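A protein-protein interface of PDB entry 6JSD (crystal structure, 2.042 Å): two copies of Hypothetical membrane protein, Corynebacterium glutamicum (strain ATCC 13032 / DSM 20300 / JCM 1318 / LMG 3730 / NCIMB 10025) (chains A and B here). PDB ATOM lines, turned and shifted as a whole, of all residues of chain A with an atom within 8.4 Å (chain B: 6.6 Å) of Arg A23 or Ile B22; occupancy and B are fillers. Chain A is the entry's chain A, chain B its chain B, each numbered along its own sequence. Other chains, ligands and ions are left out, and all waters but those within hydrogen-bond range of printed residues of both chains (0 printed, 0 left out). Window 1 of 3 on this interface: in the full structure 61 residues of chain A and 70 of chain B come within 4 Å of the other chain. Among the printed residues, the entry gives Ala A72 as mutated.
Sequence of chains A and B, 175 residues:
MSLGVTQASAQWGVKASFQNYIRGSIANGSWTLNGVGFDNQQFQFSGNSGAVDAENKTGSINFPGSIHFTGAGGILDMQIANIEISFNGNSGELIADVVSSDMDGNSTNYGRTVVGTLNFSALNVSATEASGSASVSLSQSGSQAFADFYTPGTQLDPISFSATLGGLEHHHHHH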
ATOM      1  N   LYS A  15       6.952  -9.821 -36.257  1.00  0.00           N
ATOM      2  CA  LYS A  15       7.423 -10.896 -35.377  1.00  0.00           C
ATOM      3  C   LYS A  15       7.799 -10.390 -33.981  1.00  0.00           C
ATOM      4  O   LYS A  15       7.542 -11.072 -32.979  1.00  0.00           O
ATOM      5  CB  LYS A  15       8.619 -11.619 -36.010  1.00  0.00           C
ATOM      6  CG  LYS A  15       8.264 -12.453 -37.236  1.00  0.00           C
ATOM      7  CD  LYS A  15       9.414 -13.374 -37.635  1.00  0.00           C
ATOM      8  CE  LYS A  15       9.178 -13.924 -39.038  1.00  0.00           C
ATOM      9  NZ  LYS A  15      10.375 -14.647 -39.574  1.00  0.00           N
ATOM     10  N   ALA A  16       8.430  -9.215 -33.889  1.00  0.00           N
ATOM     11  CA  ALA A  16       8.732  -8.645 -32.573  1.00  0.00           C
ATOM     12  C   ALA A  16       7.466  -8.446 -31.734  1.00  0.00           C
ATOM     13  O   ALA A  16       7.476  -8.689 -30.522  1.00  0.00           O
ATOM     14  CB  ALA A  16       9.457  -7.313 -32.724  1.00  0.00           C
ATOM     15  N   SER A  17       6.378  -7.973 -32.356  1.00  0.00           N
ATOM     16  CA  SER A  17       5.143  -7.759 -31.603  1.00  0.00           C
ATOM     17  C   SER A  17       4.546  -9.083 -31.128  1.00  0.00           C
ATOM     18  O   SER A  17       3.976  -9.150 -30.031  1.00  0.00           O
ATOM     19  CB  SER A  17       4.125  -6.969 -32.438  1.00  0.00           C
ATOM     20  OG  SER A  17       4.481  -5.587 -32.490  1.00  0.00           O
ATOM     21  N   PHE A  18       4.668 -10.152 -31.927  1.00  0.00           N
ATOM     22  CA  PHE A  18       4.193 -11.456 -31.453  1.00  0.00           C
ATOM     23  C   PHE A  18       5.051 -11.957 -30.296  1.00  0.00           C
ATOM     24  O   PHE A  18       4.529 -12.544 -29.340  1.00  0.00           O
ATOM     25  CB  PHE A  18       4.161 -12.490 -32.586  1.00  0.00           C
ATOM     26  CG  PHE A  18       2.944 -12.371 -33.484  1.00  0.00           C
ATOM     27  CD1 PHE A  18       1.685 -12.208 -32.944  1.00  0.00           C
ATOM     28  CD2 PHE A  18       3.067 -12.418 -34.862  1.00  0.00           C
ATOM     29  CE1 PHE A  18       0.562 -12.084 -33.775  1.00  0.00           C
ATOM     30  CE2 PHE A  18       1.954 -12.294 -35.701  1.00  0.00           C
ATOM     31  CZ  PHE A  18       0.698 -12.122 -35.150  1.00  0.00           C
ATOM     32  N   GLN A  19       6.369 -11.711 -30.347  1.00  0.00           N
ATOM     33  CA  GLN A  19       7.198 -12.079 -29.207  1.00  0.00           C
ATOM     34  C   GLN A  19       6.857 -11.230 -27.984  1.00  0.00           C
ATOM     35  O   GLN A  19       6.767 -11.761 -26.870  1.00  0.00           O
ATOM     36  CB  GLN A  19       8.682 -11.960 -29.571  1.00  0.00           C
ATOM     37  CG  GLN A  19       9.107 -12.931 -30.676  1.00  0.00           C
ATOM     38  CD  GLN A  19      10.602 -12.910 -30.917  1.00  0.00           C
ATOM     39  OE1 GLN A  19      11.233 -11.862 -30.830  1.00  0.00           O
ATOM     40  NE2 GLN A  19      11.177 -14.071 -31.202  1.00  0.00           N
ATOM     41  N   ASN A  20       6.667  -9.913 -28.174  1.00  0.00           N
ATOM     42  CA  ASN A  20       6.281  -9.021 -27.074  1.00  0.00           C
ATOM     43  C   ASN A  20       4.936  -9.427 -26.469  1.00  0.00           C
ATOM     44  O   ASN A  20       4.726  -9.282 -25.258  1.00  0.00           O
ATOM     45  CB  ASN A  20       6.223  -7.555 -27.548  1.00  0.00           C
ATOM     46  CG  ASN A  20       7.598  -6.999 -27.959  1.00  0.00           C
ATOM     47  OD1 ASN A  20       8.634  -7.558 -27.601  1.00  0.00           O
ATOM     48  ND2 ASN A  20       7.602  -5.891 -28.707  1.00  0.00           N
ATOM     49  N   TYR A  21       4.021  -9.946 -27.283  1.00  0.00           N
ATOM     50  CA  TYR A  21       2.768 -10.447 -26.732  1.00  0.00           C
ATOM     51  C   TYR A  21       3.020 -11.606 -25.769  1.00  0.00           C
ATOM     52  O   TYR A  21       2.533 -11.601 -24.629  1.00  0.00           O
ATOM     53  CB  TYR A  21       1.830 -10.872 -27.854  1.00  0.00           C
ATOM     54  CG  TYR A  21       0.458 -11.253 -27.324  1.00  0.00           C
ATOM     55  CD1 TYR A  21      -0.466 -10.267 -26.979  1.00  0.00           C
ATOM     56  CD2 TYR A  21       0.097 -12.586 -27.141  1.00  0.00           C
ATOM     57  CE1 TYR A  21      -1.719 -10.597 -26.480  1.00  0.00           C
ATOM     58  CE2 TYR A  21      -1.172 -12.925 -26.640  1.00  0.00           C
ATOM     59  CZ  TYR A  21      -2.068 -11.920 -26.313  1.00  0.00           C
ATOM     60  OH  TYR A  21      -3.320 -12.226 -25.817  1.00  0.00           O
ATOM     61  N   ILE A  22       3.785 -12.609 -26.218  1.00  0.00           N
ATOM     62  CA  ILE A  22       4.143 -13.742 -25.362  1.00  0.00           C
ATOM     63  C   ILE A  22       4.939 -13.280 -24.146  1.00  0.00           C
ATOM     64  O   ILE A  22       4.753 -13.796 -23.038  1.00  0.00           O
ATOM     65  CB  ILE A  22       4.922 -14.794 -26.169  1.00  0.00           C
ATOM     66  CG1 ILE A  22       4.137 -15.193 -27.408  1.00  0.00           C
ATOM     67  CG2 ILE A  22       5.197 -16.019 -25.315  1.00  0.00           C
ATOM     68  CD1 ILE A  22       4.912 -16.065 -28.318  1.00  0.00           C
ATOM     69  N   ARG A  23       5.849 -12.317 -24.330  1.00  0.00           N
ATOM     70  CA  ARG A  23       6.580 -11.783 -23.181  1.00  0.00           C
ATOM     71  C   ARG A  23       5.615 -11.214 -22.140  1.00  0.00           C
ATOM     72  O   ARG A  23       5.834 -11.354 -20.929  1.00  0.00           O
ATOM     73  CB  ARG A  23       7.572 -10.707 -23.627  1.00  0.00           C
ATOM     74  CG  ARG A  23       8.464 -10.190 -22.498  1.00  0.00           C
ATOM     75  CD  ARG A  23       8.864  -8.720 -22.666  1.00  0.00           C
ATOM     76  NE  ARG A  23       9.116  -8.080 -21.372  1.00  0.00           N
ATOM     77  CZ  ARG A  23       8.190  -7.451 -20.648  1.00  0.00           C
ATOM     78  NH1 ARG A  23       6.934  -7.359 -21.086  1.00  0.00           N
ATOM     79  NH2 ARG A  23       8.518  -6.912 -19.477  1.00  0.00           N
ATOM     80  N   GLY A  24       4.537 -10.579 -22.602  1.00  0.00           N
ATOM     81  CA  GLY A  24       3.554 -10.026 -21.684  1.00  0.00           C
ATOM     82  C   GLY A  24       2.847 -11.082 -20.854  1.00  0.00           C
ATOM     83  O   GLY A  24       2.479 -10.833 -19.703  1.00  0.00           O
ATOM     84  N   SER A  25       2.644 -12.275 -21.423  1.00  0.00           N
ATOM     85  CA  SER A  25       1.988 -13.338 -20.657  1.00  0.00           C
ATOM     86  C   SER A  25       2.916 -13.931 -19.599  1.00  0.00           C
ATOM     87  O   SER A  25       2.461 -14.324 -18.514  1.00  0.00           O
ATOM     88  CB  SER A  25       1.503 -14.435 -21.595  1.00  0.00           C
ATOM     89  OG  SER A  25       2.624 -15.053 -22.212  1.00  0.00           O
ATOM     90  N   ILE A  26       4.217 -13.998 -19.883  1.00  0.00           N
ATOM     91  CA  ILE A  26       5.154 -14.426 -18.850  1.00  0.00           C
ATOM     92  C   ILE A  26       5.187 -13.387 -17.741  1.00  0.00           C
ATOM     93  O   ILE A  26       5.075 -13.717 -16.556  1.00  0.00           O
ATOM     94  CB  ILE A  26       6.542 -14.688 -19.465  1.00  0.00           C
ATOM     95  CG1 ILE A  26       6.451 -15.940 -20.351  1.00  0.00           C
ATOM     96  CG2 ILE A  26       7.627 -14.808 -18.359  1.00  0.00           C
ATOM     97  CD1 ILE A  26       7.440 -16.005 -21.467  1.00  0.00           C
ATOM     98  N   ALA A  27       5.266 -12.105 -18.121  1.00  0.00           N
ATOM     99  CA  ALA A  27       5.335 -11.033 -17.133  1.00  0.00           C
ATOM    100  C   ALA A  27       4.085 -11.003 -16.257  1.00  0.00           C
ATOM    101  O   ALA A  27       4.171 -10.739 -15.053  1.00  0.00           O
ATOM    102  CB  ALA A  27       5.555  -9.687 -17.833  1.00  0.00           C
ATOM    103  N   ASN A  28       2.911 -11.282 -16.834  1.00  0.00           N
ATOM    104  CA  ASN A  28       1.692 -11.393 -16.041  1.00  0.00           C
ATOM    105  C   ASN A  28       1.453 -12.797 -15.499  1.00  0.00           C
ATOM    106  O   ASN A  28       0.320 -13.115 -15.133  1.00  0.00           O
ATOM    107  CB  ASN A  28       0.463 -10.954 -16.847  1.00  0.00           C
ATOM    108  CG  ASN A  28       0.552  -9.522 -17.301  1.00  0.00           C
ATOM    109  OD1 ASN A  28       0.318  -9.220 -18.470  1.00  0.00           O
ATOM    110  ND2 ASN A  28       0.924  -8.632 -16.388  1.00  0.00           N
ATOM    111  N   GLY A  29       2.481 -13.636 -15.429  1.00  0.00           N
ATOM    112  CA  GLY A  29       2.337 -14.952 -14.848  1.00  0.00           C
ATOM    113  C   GLY A  29       2.369 -14.913 -13.329  1.00  0.00           C
ATOM    114  O   GLY A  29       2.386 -13.857 -12.694  1.00  0.00           O
ATOM    115  N   PHE A  69       5.821 -22.047 -11.788  1.00  0.00           N
ATOM    116  CA  PHE A  69       5.419 -20.942 -12.642  1.00  0.00           C
ATOM    117  C   PHE A  69       4.167 -21.309 -13.432  1.00  0.00           C
ATOM    118  O   PHE A  69       4.033 -22.436 -13.909  1.00  0.00           O
ATOM    119  CB  PHE A  69       6.523 -20.522 -13.627  1.00  0.00           C
ATOM    120  CG  PHE A  69       6.140 -19.340 -14.484  1.00  0.00           C
ATOM    121  CD1 PHE A  69       6.143 -18.062 -13.957  1.00  0.00           C
ATOM    122  CD2 PHE A  69       5.762 -19.515 -15.805  1.00  0.00           C
ATOM    123  CE1 PHE A  69       5.770 -16.965 -14.730  1.00  0.00           C
ATOM    124  CE2 PHE A  69       5.376 -18.424 -16.596  1.00  0.00           C
ATOM    125  CZ  PHE A  69       5.386 -17.151 -16.059  1.00  0.00           C
ATOM    126  N   ALA A  72       0.173 -16.301 -17.646  1.00  0.00           N
ATOM    127  CA  ALA A  72      -1.200 -15.841 -17.790  1.00  0.00           C
ATOM    128  C   ALA A  72      -1.907 -16.706 -18.823  1.00  0.00           C
ATOM    129  O   ALA A  72      -1.376 -16.952 -19.909  1.00  0.00           O
ATOM    130  CB  ALA A  72      -1.240 -14.366 -18.195  1.00  0.00           C
ATOM    131  N   LEU A  76       1.448 -22.138 -20.138  1.00  0.00           N
ATOM    132  CA  LEU A  76       2.773 -22.453 -19.623  1.00  0.00           C
ATOM    133  C   LEU A  76       2.625 -22.779 -18.143  1.00  0.00           C
ATOM    134  O   LEU A  76       2.183 -21.931 -17.366  1.00  0.00           O
ATOM    135  CB  LEU A  76       3.711 -21.270 -19.845  1.00  0.00           C
ATOM    136  CG  LEU A  76       5.204 -21.542 -19.722  1.00  0.00           C
ATOM    137  CD1 LEU A  76       5.569 -22.751 -20.564  1.00  0.00           C
ATOM    138  CD2 LEU A  76       5.995 -20.312 -20.159  1.00  0.00           C
ATOM    139  N   TYR A 150      11.675 -27.539 -26.467  1.00  0.00           N
ATOM    140  CA  TYR A 150      12.983 -27.205 -27.002  1.00  0.00           C
ATOM    141  C   TYR A 150      13.754 -28.478 -27.300  1.00  0.00           C
ATOM    142  O   TYR A 150      13.664 -29.458 -26.554  1.00  0.00           O
ATOM    143  CB  TYR A 150      13.757 -26.341 -26.015  1.00  0.00           C
ATOM    144  CG  TYR A 150      12.851 -25.561 -25.101  1.00  0.00           C
ATOM    145  CD1 TYR A 150      12.321 -24.336 -25.491  1.00  0.00           C
ATOM    146  CD2 TYR A 150      12.510 -26.054 -23.851  1.00  0.00           C
ATOM    147  CE1 TYR A 150      11.480 -23.618 -24.651  1.00  0.00           C
ATOM    148  CE2 TYR A 150      11.674 -25.345 -23.004  1.00  0.00           C
ATOM    149  CZ  TYR A 150      11.160 -24.130 -23.409  1.00  0.00           C
ATOM    150  OH  TYR A 150      10.329 -23.435 -22.562  1.00  0.00           O
ATOM    151  N   SER B  17      15.832 -19.338 -20.411  1.00  0.00           N
ATOM    152  CA  SER B  17      14.782 -20.299 -20.736  1.00  0.00           C
ATOM    153  C   SER B  17      13.541 -19.596 -21.270  1.00  0.00           C
ATOM    154  O   SER B  17      12.946 -20.038 -22.262  1.00  0.00           O
ATOM    155  CB  SER B  17      14.440 -21.141 -19.507  1.00  0.00           C
ATOM    156  OG  SER B  17      15.542 -21.933 -19.127  1.00  0.00           O
ATOM    157  N   PHE B  18      13.134 -18.493 -20.629  1.00  0.00           N
ATOM    158  CA  PHE B  18      11.981 -17.733 -21.114  1.00  0.00           C
ATOM    159  C   PHE B  18      12.233 -17.182 -22.508  1.00  0.00           C
ATOM    160  O   PHE B  18      11.350 -17.229 -23.378  1.00  0.00           O
ATOM    161  CB  PHE B  18      11.659 -16.597 -20.151  1.00  0.00           C
ATOM    162  CG  PHE B  18      10.851 -17.021 -18.959  1.00  0.00           C
ATOM    163  CD1 PHE B  18       9.777 -17.895 -19.108  1.00  0.00           C
ATOM    164  CD2 PHE B  18      11.163 -16.549 -17.685  1.00  0.00           C
ATOM    165  CE1 PHE B  18       9.014 -18.277 -17.998  1.00  0.00           C
ATOM    166  CE2 PHE B  18      10.409 -16.920 -16.574  1.00  0.00           C
ATOM    167  CZ  PHE B  18       9.329 -17.787 -16.727  1.00  0.00           C
ATOM    168  N   GLN B  19      13.445 -16.670 -22.749  1.00  0.00           N
ATOM    169  CA  GLN B  19      13.787 -16.214 -24.090  1.00  0.00           C
ATOM    170  C   GLN B  19      13.678 -17.349 -25.102  1.00  0.00           C
ATOM    171  O   GLN B  19      13.101 -17.169 -26.184  1.00  0.00           O
ATOM    172  CB  GLN B  19      15.190 -15.614 -24.113  1.00  0.00           C
ATOM    173  CG  GLN B  19      15.479 -14.870 -25.404  1.00  0.00           C
ATOM    174  CD  GLN B  19      14.692 -13.565 -25.527  1.00  0.00           C
ATOM    175  OE1 GLN B  19      13.481 -13.557 -25.819  1.00  0.00           O
ATOM    176  NE2 GLN B  19      15.386 -12.447 -25.313  1.00  0.00           N
ATOM    177  N   ASN B  20      14.205 -18.532 -24.755  1.00  0.00           N
ATOM    178  CA  ASN B  20      14.035 -19.709 -25.606  1.00  0.00           C
ATOM    179  C   ASN B  20      12.559 -19.970 -25.903  1.00  0.00           C
ATOM    180  O   ASN B  20      12.180 -20.220 -27.057  1.00  0.00           O
ATOM    181  CB  ASN B  20      14.665 -20.943 -24.946  1.00  0.00           C
ATOM    182  CG  ASN B  20      16.192 -20.896 -24.932  1.00  0.00           C
ATOM    183  OD1 ASN B  20      16.809 -20.059 -25.587  1.00  0.00           O
ATOM    184  ND2 ASN B  20      16.799 -21.799 -24.177  1.00  0.00           N
ATOM    185  N   TYR B  21      11.709 -19.895 -24.877  1.00  0.00           N
ATOM    186  CA  TYR B  21      10.284 -20.126 -25.082  1.00  0.00           C
ATOM    187  C   TYR B  21       9.675 -19.064 -26.001  1.00  0.00           C
ATOM    188  O   TYR B  21       8.880 -19.387 -26.897  1.00  0.00           O
ATOM    189  CB  TYR B  21       9.565 -20.162 -23.732  1.00  0.00           C
ATOM    190  CG  TYR B  21       8.070 -20.361 -23.851  1.00  0.00           C
ATOM    191  CD1 TYR B  21       7.526 -21.636 -23.971  1.00  0.00           C
ATOM    192  CD2 TYR B  21       7.205 -19.277 -23.866  1.00  0.00           C
ATOM    193  CE1 TYR B  21       6.152 -21.827 -24.087  1.00  0.00           C
ATOM    194  CE2 TYR B  21       5.835 -19.453 -23.985  1.00  0.00           C
ATOM    195  CZ  TYR B  21       5.312 -20.732 -24.093  1.00  0.00           C
ATOM    196  OH  TYR B  21       3.950 -20.916 -24.213  1.00  0.00           O
ATOM    197  N   ILE B  22      10.055 -17.797 -25.809  1.00  0.00           N
ATOM    198  CA  ILE B  22       9.476 -16.712 -26.595  1.00  0.00           C
ATOM    199  C   ILE B  22       9.927 -16.803 -28.050  1.00  0.00           C
ATOM    200  O   ILE B  22       9.107 -16.732 -28.974  1.00  0.00           O
ATOM    201  CB  ILE B  22       9.829 -15.351 -25.969  1.00  0.00           C
ATOM    202  CG1 ILE B  22       9.117 -15.185 -24.619  1.00  0.00           C
ATOM    203  CG2 ILE B  22       9.496 -14.213 -26.930  1.00  0.00           C
ATOM    204  CD1 ILE B  22       9.578 -13.960 -23.838  1.00  0.00           C
ATOM    205  N   ARG B  23      11.239 -16.958 -28.278  1.00  0.00           N
ATOM    206  CA  ARG B  23      11.743 -17.111 -29.638  1.00  0.00           C
ATOM    207  C   ARG B  23      11.247 -18.407 -30.264  1.00  0.00           C
ATOM    208  O   ARG B  23      10.883 -18.436 -31.449  1.00  0.00           O
ATOM    209  CB  ARG B  23      13.275 -17.082 -29.651  1.00  0.00           C
ATOM    210  CG  ARG B  23      13.910 -15.736 -29.381  1.00  0.00           C
ATOM    211  CD  ARG B  23      15.424 -15.870 -29.443  1.00  0.00           C
ATOM    212  NE  ARG B  23      16.126 -14.693 -28.942  1.00  0.00           N
ATOM    213  CZ  ARG B  23      17.451 -14.564 -28.934  1.00  0.00           C
ATOM    214  NH1 ARG B  23      18.216 -15.541 -29.406  1.00  0.00           N
ATOM    215  NH2 ARG B  23      18.013 -13.461 -28.455  1.00  0.00           N
ATOM    216  N   GLY B  24      11.247 -19.496 -29.487  1.00  0.00           N
ATOM    217  CA  GLY B  24      10.794 -20.773 -30.018  1.00  0.00           C
ATOM    218  C   GLY B  24       9.362 -20.726 -30.526  1.00  0.00           C
ATOM    219  O   GLY B  24       9.040 -21.328 -31.554  1.00  0.00           O
ATOM    220  N   SER B  25       8.488 -20.000 -29.819  1.00  0.00           N
ATOM    221  CA  SER B  25       7.072 -19.968 -30.185  1.00  0.00           C
ATOM    222  C   SER B  25       6.861 -19.374 -31.576  1.00  0.00           C
ATOM    223  O   SER B  25       5.947 -19.789 -32.304  1.00  0.00           O
ATOM    224  CB  SER B  25       6.272 -19.173 -29.145  1.00  0.00           C
ATOM    225  OG  SER B  25       6.287 -19.790 -27.863  1.00  0.00           O
ATOM    226  N   ILE B  26       7.663 -18.371 -31.948  1.00  0.00           N
ATOM    227  CA  ILE B  26       7.488 -17.733 -33.252  1.00  0.00           C
ATOM    228  C   ILE B  26       8.213 -18.526 -34.329  1.00  0.00           C
ATOM    229  O   ILE B  26       7.687 -18.714 -35.435  1.00  0.00           O
ATOM    230  CB  ILE B  26       7.965 -16.261 -33.224  1.00  0.00           C
ATOM    231  CG1 ILE B  26       6.889 -15.338 -32.657  1.00  0.00           C
ATOM    232  CG2 ILE B  26       8.305 -15.765 -34.632  1.00  0.00           C
ATOM    233  CD1 ILE B  26       6.664 -15.499 -31.209  1.00  0.00           C
ATOM    234  N   ALA B  27       9.420 -19.015 -34.005  1.00  0.00           N
ATOM    235  CA  ALA B  27      10.275 -19.674 -34.988  1.00  0.00           C
ATOM    236  C   ALA B  27       9.690 -21.005 -35.452  1.00  0.00           C
ATOM    237  O   ALA B  27       9.827 -21.372 -36.626  1.00  0.00           O
ATOM    238  CB  ALA B  27      11.672 -19.889 -34.398  1.00  0.00           C
ATOM    239  N   GLN B 144       5.298  -3.090 -17.087  1.00  0.00           N
ATOM    240  CA  GLN B 144       5.654  -4.417 -16.609  1.00  0.00           C
ATOM    241  C   GLN B 144       7.119  -4.464 -16.177  1.00  0.00           C
ATOM    242  O   GLN B 144       7.754  -5.523 -16.203  1.00  0.00           O
ATOM    243  CB  GLN B 144       5.352  -5.468 -17.676  1.00  0.00           C
ATOM    244  CG  GLN B 144       3.860  -5.716 -17.887  1.00  0.00           C
ATOM    245  CD  GLN B 144       3.580  -6.414 -19.199  1.00  0.00           C
ATOM    246  OE1 GLN B 144       4.380  -6.347 -20.134  1.00  0.00           O
ATOM    247  NE2 GLN B 144       2.436  -7.086 -19.281  1.00  0.00           N
ATOM    248  N   ALA B 145       7.656  -3.305 -15.784  1.00  0.00           N
ATOM    249  CA  ALA B 145       9.051  -3.218 -15.367  1.00  0.00           C
ATOM    250  C   ALA B 145       9.331  -4.123 -14.176  1.00  0.00           C
ATOM    251  O   ALA B 145      10.468  -4.587 -14.003  1.00  0.00           O
ATOM    252  CB  ALA B 145       9.405  -1.767 -15.036  1.00  0.00           C
ATOM    253  N   ALA B 147       8.711  -7.052 -13.892  1.00  0.00           N
ATOM    254  CA  ALA B 147       9.087  -8.369 -14.385  1.00  0.00           C
ATOM    255  C   ALA B 147      10.472  -8.399 -15.024  1.00  0.00           C
ATOM    256  O   ALA B 147      10.895  -9.463 -15.491  1.00  0.00           O
ATOM    257  CB  ALA B 147       8.048  -8.861 -15.400  1.00  0.00           C
ATOM    258  N   ASP B 148      11.174  -7.261 -15.057  1.00  0.00           N
ATOM    259  CA  ASP B 148      12.475  -7.171 -15.720  1.00  0.00           C
ATOM    260  C   ASP B 148      13.523  -8.095 -15.106  1.00  0.00           C
ATOM    261  O   ASP B 148      14.520  -8.407 -15.769  1.00  0.00           O
ATOM    262  CB  ASP B 148      12.994  -5.722 -15.679  1.00  0.00           C
ATOM    263  CG  ASP B 148      12.205  -4.780 -16.584  1.00  0.00           C
ATOM    264  OD1 ASP B 148      11.357  -5.265 -17.361  1.00  0.00           O
ATOM    265  OD2 ASP B 148      12.441  -3.553 -16.519  1.00  0.00           O
ATOM    266  N   THR B 151      12.018 -11.590 -16.740  1.00  0.00           N
ATOM    267  CA  THR B 151      11.540 -11.645 -18.116  1.00  0.00           C
ATOM    268  C   THR B 151      12.512 -10.925 -19.034  1.00  0.00           C
ATOM    269  O   THR B 151      12.850  -9.765 -18.769  1.00  0.00           O
ATOM    270  CB  THR B 151      10.150 -11.006 -18.251  1.00  0.00           C
ATOM    271  OG1 THR B 151       9.318 -11.348 -17.132  1.00  0.00           O
ATOM    272  CG2 THR B 151       9.484 -11.499 -19.512  1.00  0.00           C
ATOM    273  N   PRO B 152      12.962 -11.548 -20.125  1.00  0.00           N
ATOM    274  CA  PRO B 152      13.723 -10.798 -21.133  1.00  0.00           C
ATOM    275  C   PRO B 152      12.967  -9.553 -21.585  1.00  0.00           C
ATOM    276  O   PRO B 152      11.732  -9.513 -21.584  1.00  0.00           O
ATOM    277  CB  PRO B 152      13.888 -11.807 -22.280  1.00  0.00           C
ATOM    278  CG  PRO B 152      12.840 -12.862 -22.040  1.00  0.00           C
ATOM    279  CD  PRO B 152      12.717 -12.940 -20.538  1.00  0.00           C
ATOM    280  N   GLY B 153      13.724  -8.524 -21.964  1.00  0.00           N
ATOM    281  CA  GLY B 153      13.132  -7.268 -22.378  1.00  0.00           C
ATOM    282  C   GLY B 153      12.414  -7.357 -23.718  1.00  0.00           C
ATOM    283  O   GLY B 153      12.568  -8.299 -24.504  1.00  0.00           O
ATOM    284  N   THR B 154      11.612  -6.331 -23.986  1.00  0.00           N
ATOM    285  CA  THR B 154      10.867  -6.290 -25.238  1.00  0.00           C
ATOM    286  C   THR B 154      11.803  -6.026 -26.407  1.00  0.00           C
ATOM    287  O   THR B 154      12.909  -5.502 -26.248  1.00  0.00           O
ATOM    288  CB  THR B 154       9.801  -5.195 -25.212  1.00  0.00           C
ATOM    289  OG1 THR B 154      10.445  -3.922 -25.115  1.00  0.00           O
ATOM    290  CG2 THR B 154       8.849  -5.392 -24.024  1.00  0.00           C
ATOM    291  N   GLN B 155      11.334  -6.382 -27.595  1.00  0.00           N
ATOM    292  CA  GLN B 155      12.065  -6.184 -28.837  1.00  0.00           C
ATOM    293  C   GLN B 155      11.414  -5.063 -29.640  1.00  0.00           C
ATOM    294  O   GLN B 155      10.180  -4.969 -29.691  1.00  0.00           O
ATOM    295  CB  GLN B 155      12.062  -7.478 -29.648  1.00  0.00           C
ATOM    296  CG  GLN B 155      13.241  -7.652 -30.549  1.00  0.00           C
ATOM    297  CD  GLN B 155      13.423  -9.089 -30.927  1.00  0.00           C
ATOM    298  OE1 GLN B 155      12.622  -9.646 -31.673  1.00  0.00           O
ATOM    299  NE2 GLN B 155      14.465  -9.714 -30.395  1.00  0.00           N
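OE1 of Gln B155 sits close to OE1 of Gln A19 (2.7 Å). O of Gln B155 lies within hydrogen-bond range of ND2 of Asn A20 (2.9 Å). The side-chain amide oxygen (OE1) of Gln B144 lies within hydrogen-bond range of the guanidinium group (NH1) of Arg A23 (2.9 Å). The side-chain carboxylate of Asp B148 lies within salt-bridge range of the guanidinium group of Arg A23 (3.9 Å). The guanidinium group of Arg A23 sits at hydrogen-bond distance from the backbone carbonyl oxygen of Pro B152, at 3.0 Å. The side-chain amide oxygen (OD1) of Asn A28 is in hydrogen-bond range of the side-chain amide nitrogen (NE2) of Gln B144 (3.1 Å).
The backbone carbonyl oxygen (O) of Ala A16 lies close to the side-chain amide nitrogen (ND2) of Asn A20. O of Ile A22 sits at hydrogen-bond distance from OG of Ser A25. OD1 of Asn A28 lies close to O of Gly A24, at 3.0 Å. OG of Ser B25 is in hydrogen-bond range of O of Tyr B21 (2.8 Å). OG1 of Thr B151 is in hydrogen-bond range of O of Ala B147, 3.0 Å away.
Among the printed residues, pairs that only touch across the chains: Arg A23 with Thr B151, Ile A22 with Ile B26, Gln A19 with Arg B23, Asn A20 with Thr B154, Ile A22 with Ser B25, Tyr A150 with Tyr B21, Gln A19 with Ile B22, Ala A27 with Ala B147, Gln A19 with Ile B26, Arg A23 with Thr B154, Ile A26 with Ile B22, Leu A76 with Tyr B21, Ile A22 with Tyr B21, Ile A26 with Phe B18, Arg A23 with Ile B22, Gly A24 with Gln B144, Ala A16 with Gln B155, Phe A69 with Phe B18, Phe A18 with Ile B26, Arg A23 with Gly B153, Ile A26 with Thr B151, Ala A27 with Thr B151 and Lys A15 with Ile B26.
Arg A23 touches seven residues of chain B. Of the printed residues of chain B, Ala A27 touches Ala B147 (3.6 Å) and Thr B151 (3.995 Å). Ala A72 touches none of the printed residues of chain B. Ile B22 touches just these residues of chain A: Gln A19 (3.6 Å), Arg A23 (3.8 Å) and Ile A26 (3.7 Å). Of the printed residues of chain A, Gln B144 touches Arg A23, Gly A24 and Asn A28. Printed residues of chain A within 4 Å of Asp B148: Arg A23 (3.9 Å). Of the printed residues of chain A, Gly B153 touches Arg A23. The nearest residue of chain A that does not touch Ile B22 is Ile A22 (4.1 Å).
Hydrophobic or aromatic side chains of chain A that line the printed part of chain B: Ala A16, Phe A18, Ile A22, Ile A26, Ala A27, Phe A69, Leu A76 and Tyr A150. Of the 20 printed residues of chain B, 14 touch a printed residue of chain A. Printed residues of chain B that touch a printed residue of chain A: Phe B18, Tyr B21, Ile B22, Arg B23, Ser B25, Ile B26, Gln B144, Ala B147, Asp B148, Thr B151, Pro B152, Gly B153, Thr B154 and Gln B155. Hydrophobic or aromatic side chains of chain B within 4 Å of the printed part of chain A: Phe B18, Tyr B21, Ile B22, Ile B26 and Ala B147. Among the printed residues, 29 pairs touch across the chains. Among the printed residues, Asp or Glu carboxylates within 4 Å of a Lys or Arg side-chain nitrogen of the other chain: Arg A23 with Asp B148 (3.9 Å).
Gln A19 touches Arg B23, but with the chains exchanged Arg A23 does not touch Gln B19 (6.9 Å). Ile A22 touches Ile B26, and with the chains exchanged Ile A26 touches Ile B22. Arg A23 touches Ile B22, but with the chains exchanged Ile A22 does not touch Arg B23 (6.4 Å). Positions printed for both chains: 17, 18, 19, 20, 21, 22, 23, 24, 25, 26 and 27.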
